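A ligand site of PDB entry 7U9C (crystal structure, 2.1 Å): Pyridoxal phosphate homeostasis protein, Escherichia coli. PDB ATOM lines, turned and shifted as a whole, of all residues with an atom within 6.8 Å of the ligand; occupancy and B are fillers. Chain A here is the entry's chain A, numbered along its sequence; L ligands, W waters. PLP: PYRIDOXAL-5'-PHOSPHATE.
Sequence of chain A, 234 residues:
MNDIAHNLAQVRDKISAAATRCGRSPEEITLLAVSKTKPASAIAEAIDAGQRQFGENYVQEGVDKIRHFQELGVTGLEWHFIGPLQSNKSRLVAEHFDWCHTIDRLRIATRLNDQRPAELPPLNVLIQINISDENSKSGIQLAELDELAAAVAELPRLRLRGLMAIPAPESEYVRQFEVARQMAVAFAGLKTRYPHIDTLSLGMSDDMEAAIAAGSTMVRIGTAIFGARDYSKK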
ATOM      1  N   LEU A  32      20.655  14.750 -21.447  1.00  0.00           N
ATOM      2  CA  LEU A  32      21.177  13.607 -20.712  1.00  0.00           C
ATOM      3  C   LEU A  32      20.094  12.533 -20.668  1.00  0.00           C
ATOM      4  O   LEU A  32      19.043  12.727 -20.031  1.00  0.00           O
ATOM      5  CB  LEU A  32      21.610  14.001 -19.298  1.00  0.00           C
ATOM      6  CG  LEU A  32      22.248  12.891 -18.442  1.00  0.00           C
ATOM      7  CD1 LEU A  32      23.537  12.405 -19.066  1.00  0.00           C
ATOM      8  CD2 LEU A  32      22.497  13.331 -16.978  1.00  0.00           C
ATOM      9  N   VAL A  34      18.556   9.454 -19.209  1.00  0.00           N
ATOM     10  CA  VAL A  34      18.663   8.792 -17.913  1.00  0.00           C
ATOM     11  C   VAL A  34      18.194   7.360 -18.072  1.00  0.00           C
ATOM     12  O   VAL A  34      16.999   7.108 -18.264  1.00  0.00           O
ATOM     13  CB  VAL A  34      17.864   9.538 -16.830  1.00  0.00           C
ATOM     14  CG1 VAL A  34      17.867   8.757 -15.519  1.00  0.00           C
ATOM     15  CG2 VAL A  34      18.465  10.927 -16.635  1.00  0.00           C
ATOM     16  N   LYS A  36      18.707   4.804 -15.900  1.00  0.00           N
ATOM     17  CA  LYS A  36      18.467   4.116 -14.629  1.00  0.00           C
ATOM     18  C   LYS A  36      17.326   3.113 -14.761  1.00  0.00           C
ATOM     19  O   LYS A  36      16.279   3.412 -15.328  1.00  0.00           O
ATOM     20  CB  LYS A  36      18.153   5.186 -13.555  1.00  0.00           C
ATOM     21  CG  LYS A  36      16.971   4.916 -12.651  1.00  0.00           C
ATOM     22  CD  LYS A  36      16.701   6.058 -11.677  1.00  0.00           C
ATOM     23  CE  LYS A  36      15.575   6.951 -12.169  1.00  0.00           C
ATOM     24  NZ  LYS A  36      15.633   8.301 -11.532  1.00  0.00           N
ATOM     25  N   ASN A  57      21.980   6.164 -11.768  1.00  0.00           N
ATOM     26  CA  ASN A  57      21.758   6.526 -10.373  1.00  0.00           C
ATOM     27  C   ASN A  57      22.336   5.562  -9.364  1.00  0.00           C
ATOM     28  O   ASN A  57      22.551   5.967  -8.221  1.00  0.00           O
ATOM     29  CB  ASN A  57      20.250   6.641 -10.071  1.00  0.00           C
ATOM     30  CG  ASN A  57      19.639   7.858 -10.674  1.00  0.00           C
ATOM     31  OD1 ASN A  57      19.273   8.806  -9.966  1.00  0.00           O
ATOM     32  ND2 ASN A  57      19.514   7.855 -11.992  1.00  0.00           N
ATOM     33  N   TYR A  58      22.613   4.323  -9.744  1.00  0.00           N
ATOM     34  CA  TYR A  58      23.090   3.303  -8.832  1.00  0.00           C
ATOM     35  C   TYR A  58      24.431   2.790  -9.321  1.00  0.00           C
ATOM     36  O   TYR A  58      24.586   2.504 -10.525  1.00  0.00           O
ATOM     37  CB  TYR A  58      22.065   2.185  -8.707  1.00  0.00           C
ATOM     38  CG  TYR A  58      20.677   2.752  -8.480  1.00  0.00           C
ATOM     39  CD1 TYR A  58      20.388   3.475  -7.329  1.00  0.00           C
ATOM     40  CD2 TYR A  58      19.680   2.602  -9.429  1.00  0.00           C
ATOM     41  CE1 TYR A  58      19.143   4.013  -7.116  1.00  0.00           C
ATOM     42  CE2 TYR A  58      18.420   3.139  -9.235  1.00  0.00           C
ATOM     43  CZ  TYR A  58      18.158   3.847  -8.079  1.00  0.00           C
ATOM     44  OH  TYR A  58      16.906   4.382  -7.896  1.00  0.00           O
ATOM     45  N   ILE A  82      24.354  10.445 -11.328  1.00  0.00           N
ATOM     46  CA  ILE A  82      23.392  11.433 -10.863  1.00  0.00           C
ATOM     47  C   ILE A  82      22.620  10.959  -9.634  1.00  0.00           C
ATOM     48  O   ILE A  82      21.628  11.588  -9.265  1.00  0.00           O
ATOM     49  CB  ILE A  82      22.430  11.842 -11.985  1.00  0.00           C
ATOM     50  CG1 ILE A  82      21.559  10.657 -12.401  1.00  0.00           C
ATOM     51  CG2 ILE A  82      23.196  12.407 -13.187  1.00  0.00           C
ATOM     52  CD1 ILE A  82      20.582  11.019 -13.540  1.00  0.00           C
ATOM     53  N   GLY A  83      23.034   9.856  -8.998  1.00  0.00           N
ATOM     54  CA  GLY A  83      22.429   9.394  -7.766  1.00  0.00           C
ATOM     55  C   GLY A  83      23.219   9.854  -6.543  1.00  0.00           C
ATOM     56  O   GLY A  83      24.345  10.356  -6.677  1.00  0.00           O
ATOM     57  N   THR A 102      26.332  15.101  -8.084  1.00  0.00           N
ATOM     58  CA  THR A 102      25.764  15.073  -6.742  1.00  0.00           C
ATOM     59  C   THR A 102      26.798  15.365  -5.657  1.00  0.00           C
ATOM     60  O   THR A 102      26.782  14.769  -4.575  1.00  0.00           O
ATOM     61  CB  THR A 102      25.097  13.728  -6.476  1.00  0.00           C
ATOM     62  OG1 THR A 102      26.033  12.683  -6.777  1.00  0.00           O
ATOM     63  CG2 THR A 102      23.875  13.542  -7.368  1.00  0.00           C
ATOM     64  N   MET A 164      23.828  21.461  -9.990  1.00  0.00           N
ATOM     65  CA  MET A 164      22.683  20.611 -10.287  1.00  0.00           C
ATOM     66  C   MET A 164      21.656  20.824  -9.189  1.00  0.00           C
ATOM     67  O   MET A 164      22.004  21.159  -8.056  1.00  0.00           O
ATOM     68  CB  MET A 164      23.087  19.107 -10.357  1.00  0.00           C
ATOM     69  CG  MET A 164      21.948  18.168 -10.763  1.00  0.00           C
ATOM     70  SD  MET A 164      20.946  17.554  -9.383  1.00  0.00           S
ATOM     71  CE  MET A 164      21.915  16.160  -8.813  1.00  0.00           C
ATOM     72  N   ILE A 166      17.593  19.050  -7.993  1.00  0.00           N
ATOM     73  CA  ILE A 166      16.311  18.384  -8.176  1.00  0.00           C
ATOM     74  C   ILE A 166      15.298  19.175  -7.379  1.00  0.00           C
ATOM     75  O   ILE A 166      15.179  18.959  -6.169  1.00  0.00           O
ATOM     76  CB  ILE A 166      16.345  16.926  -7.707  1.00  0.00           C
ATOM     77  CG1 ILE A 166      17.541  16.189  -8.311  1.00  0.00           C
ATOM     78  CG2 ILE A 166      15.043  16.230  -8.068  1.00  0.00           C
ATOM     79  CD1 ILE A 166      17.751  14.810  -7.705  1.00  0.00           C
ATOM     80  N   GLY A 203      16.181  20.391 -14.783  1.00  0.00           N
ATOM     81  CA  GLY A 203      15.032  20.136 -15.631  1.00  0.00           C
ATOM     82  C   GLY A 203      14.847  18.668 -15.956  1.00  0.00           C
ATOM     83  O   GLY A 203      15.812  17.985 -16.323  1.00  0.00           O
ATOM     84  N   MET A 204      13.615  18.177 -15.814  1.00  0.00           N
ATOM     85  CA  MET A 204      13.214  16.858 -16.272  1.00  0.00           C
ATOM     86  C   MET A 204      12.000  17.005 -17.194  1.00  0.00           C
ATOM     87  O   MET A 204      11.661  18.132 -17.575  1.00  0.00           O
ATOM     88  CB  MET A 204      12.913  15.961 -15.068  1.00  0.00           C
ATOM     89  CG  MET A 204      14.033  15.903 -14.022  1.00  0.00           C
ATOM     90  SD  MET A 204      13.618  14.945 -12.547  1.00  0.00           S
ATOM     91  CE  MET A 204      15.138  15.008 -11.675  1.00  0.00           C
ATOM     92  N   SER A 205      11.319  15.902 -17.544  1.00  0.00           N
ATOM     93  CA  SER A 205      10.268  15.975 -18.561  1.00  0.00           C
ATOM     94  C   SER A 205       9.174  16.982 -18.197  1.00  0.00           C
ATOM     95  O   SER A 205       8.728  17.757 -19.045  1.00  0.00           O
ATOM     96  CB  SER A 205       9.647  14.603 -18.792  1.00  0.00           C
ATOM     97  OG  SER A 205      10.569  13.746 -19.443  1.00  0.00           O
ATOM     98  N   ASP A 206       8.739  16.999 -16.946  1.00  0.00           N
ATOM     99  CA  ASP A 206       7.559  17.780 -16.610  1.00  0.00           C
ATOM    100  C   ASP A 206       7.836  19.260 -16.389  1.00  0.00           C
ATOM    101  O   ASP A 206       6.895  20.060 -16.409  1.00  0.00           O
ATOM    102  CB  ASP A 206       6.876  17.187 -15.367  1.00  0.00           C
ATOM    103  CG  ASP A 206       6.325  15.780 -15.619  1.00  0.00           C
ATOM    104  OD1 ASP A 206       5.949  15.488 -16.783  1.00  0.00           O
ATOM    105  OD2 ASP A 206       6.288  14.964 -14.669  1.00  0.00           O
ATOM    106  N   VAL A 219      19.237  18.997 -19.541  1.00  0.00           N
ATOM    107  CA  VAL A 219      18.023  18.396 -18.982  1.00  0.00           C
ATOM    108  C   VAL A 219      18.236  16.887 -18.879  1.00  0.00           C
ATOM    109  O   VAL A 219      19.046  16.298 -19.607  1.00  0.00           O
ATOM    110  CB  VAL A 219      16.760  18.728 -19.815  1.00  0.00           C
ATOM    111  CG1 VAL A 219      16.497  20.231 -19.784  1.00  0.00           C
ATOM    112  CG2 VAL A 219      16.897  18.211 -21.245  1.00  0.00           C
ATOM    113  N   ARG A 220      17.535  16.280 -17.924  1.00  0.00           N
ATOM    114  CA  ARG A 220      17.718  14.867 -17.597  1.00  0.00           C
ATOM    115  C   ARG A 220      16.407  14.152 -17.880  1.00  0.00           C
ATOM    116  O   ARG A 220      15.453  14.271 -17.099  1.00  0.00           O
ATOM    117  CB  ARG A 220      18.149  14.693 -16.137  1.00  0.00           C
ATOM    118  CG  ARG A 220      19.374  15.498 -15.761  1.00  0.00           C
ATOM    119  CD  ARG A 220      19.798  15.249 -14.314  1.00  0.00           C
ATOM    120  NE  ARG A 220      18.709  15.496 -13.369  1.00  0.00           N
ATOM    121  CZ  ARG A 220      18.431  16.687 -12.824  1.00  0.00           C
ATOM    122  NH1 ARG A 220      19.149  17.744 -13.116  1.00  0.00           N
ATOM    123  NH2 ARG A 220      17.418  16.805 -11.980  1.00  0.00           N
ATOM    124  N   ILE A 221      16.331  13.412 -18.982  1.00  0.00           N
ATOM    125  CA  ILE A 221      15.085  12.774 -19.396  1.00  0.00           C
ATOM    126  C   ILE A 221      15.255  11.260 -19.333  1.00  0.00           C
ATOM    127  O   ILE A 221      16.191  10.696 -19.920  1.00  0.00           O
ATOM    128  CB  ILE A 221      14.670  13.209 -20.820  1.00  0.00           C
ATOM    129  CG1 ILE A 221      14.724  14.741 -20.964  1.00  0.00           C
ATOM    130  CG2 ILE A 221      13.299  12.641 -21.173  1.00  0.00           C
ATOM    131  CD1 ILE A 221      13.808  15.507 -20.044  1.00  0.00           C
ATOM    132  N   GLY A 222      14.345  10.588 -18.632  1.00  0.00           N
ATOM    133  CA  GLY A 222      14.338   9.143 -18.617  1.00  0.00           C
ATOM    134  C   GLY A 222      13.101   8.549 -19.268  1.00  0.00           C
ATOM    135  O   GLY A 222      13.161   8.087 -20.418  1.00  0.00           O
ATOM    136  N   THR A 223      11.976   8.597 -18.542  1.00  0.00           N
ATOM    137  CA  THR A 223      10.724   7.952 -18.968  1.00  0.00           C
ATOM    138  C   THR A 223      10.369   8.289 -20.413  1.00  0.00           C
ATOM    139  O   THR A 223      10.037   7.397 -21.192  1.00  0.00           O
ATOM    140  CB  THR A 223       9.583   8.366 -18.030  1.00  0.00           C
ATOM    141  OG1 THR A 223       9.809   7.802 -16.742  1.00  0.00           O
ATOM    142  CG2 THR A 223       8.265   7.867 -18.567  1.00  0.00           C
ATOM    143  N   ALA A 224      10.410   9.573 -20.766  1.00  0.00           N
ATOM    144  CA  ALA A 224      10.018   9.983 -22.103  1.00  0.00           C
ATOM    145  C   ALA A 224      10.928   9.431 -23.196  1.00  0.00           C
ATOM    146  O   ALA A 224      10.584   9.538 -24.379  1.00  0.00           O
ATOM    147  CB  ALA A 224       9.977  11.509 -22.182  1.00  0.00           C
ATOM    148  N   ILE A 225      12.063   8.843 -22.852  1.00  0.00           N
ATOM    149  CA  ILE A 225      12.933   8.204 -23.837  1.00  0.00           C
ATOM    150  C   ILE A 225      12.754   6.692 -23.824  1.00  0.00           C
ATOM    151  O   ILE A 225      12.621   6.068 -24.881  1.00  0.00           O
ATOM    152  CB  ILE A 225      14.402   8.599 -23.593  1.00  0.00           C
ATOM    153  CG1 ILE A 225      14.653  10.043 -24.010  1.00  0.00           C
ATOM    154  CG2 ILE A 225      15.349   7.637 -24.317  1.00  0.00           C
ATOM    155  CD1 ILE A 225      15.999  10.572 -23.540  1.00  0.00           C
ATOM    156  N   GLY A 227      10.500   4.786 -21.809  1.00  0.00           N
ATOM    157  CA  GLY A 227       9.272   4.234 -21.292  1.00  0.00           C
ATOM    158  C   GLY A 227       9.388   3.928 -19.807  1.00  0.00           C
ATOM    159  O   GLY A 227      10.251   4.441 -19.098  1.00  0.00           O
HETATM  160  N1  PLP L   1      17.180  13.083 -13.050  1.00  0.00           N
HETATM  161  C2  PLP L   1      17.446  12.340 -11.930  1.00  0.00           C
HETATM  162  C2A PLP L   1      18.405  12.852 -10.891  1.00  0.00           C
HETATM  163  C3  PLP L   1      16.834  11.107 -11.759  1.00  0.00           C
HETATM  164  O3  PLP L   1      17.090  10.346 -10.643  1.00  0.00           O
HETATM  165  C4  PLP L   1      15.938  10.629 -12.724  1.00  0.00           C
HETATM  166  C4A PLP L   1      15.584   9.182 -12.669  1.00  0.00           C
HETATM  167  C5  PLP L   1      15.680  11.395 -13.870  1.00  0.00           C
HETATM  168  C6  PLP L   1      16.307  12.627 -14.012  1.00  0.00           C
HETATM  169  C5A PLP L   1      14.722  10.950 -14.979  1.00  0.00           C
HETATM  170  O4P PLP L   1      13.419  10.639 -14.493  1.00  0.00           O
HETATM  171  P   PLP L   1      12.076  10.509 -15.398  1.00  0.00           P
HETATM  172  O1P PLP L   1      10.890  11.044 -14.638  1.00  0.00           O
HETATM  173  O2P PLP L   1      12.216  11.256 -16.703  1.00  0.00           O
HETATM  174  O3P PLP L   1      11.886   9.056 -15.730  1.00  0.00           O
HETATM  175  O   HOH W   1      16.765  11.163  -8.199  1.00  0.00           O
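The guanidinium group (NE) of Arg 220 is in hydrogen-bond range of a nitrogen (N1) of the ligand (2.9 Å).
The side-chain amino group (NZ) of Lys 36 is covalently linked to a carbon (C4A) of the ligand.
The side-chain amide oxygen (OD1) of Asn 57 sits at hydrogen-bond distance from an oxygen (O3) of the ligand (2.8 Å).
OG1 of Thr 223 is in hydrogen-bond range of O3P of the ligand (2.6 Å).
O2P of the ligand sits at hydrogen-bond distance from N of Gly 222, 2.9 Å away.
N of Thr 223 is in hydrogen-bond range of O3P of the ligand (2.9 Å).
The backbone NH of Arg 220 sits at hydrogen-bond distance from the backbone carbonyl oxygen of Gly 203 (2.9 Å).
The backbone NH (N) of Val 34 sits at hydrogen-bond distance from the backbone carbonyl oxygen (O) of Ile 221 (2.8 Å).
Residues that only touch the ligand: Val 34 (3.7 Å), Ile 82 (3.8 Å), Ile 166 (3.8 Å) and Met 204 (3.1 Å).
Along chain A the residues within 4 Å of the ligand span positions 34 to 223.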
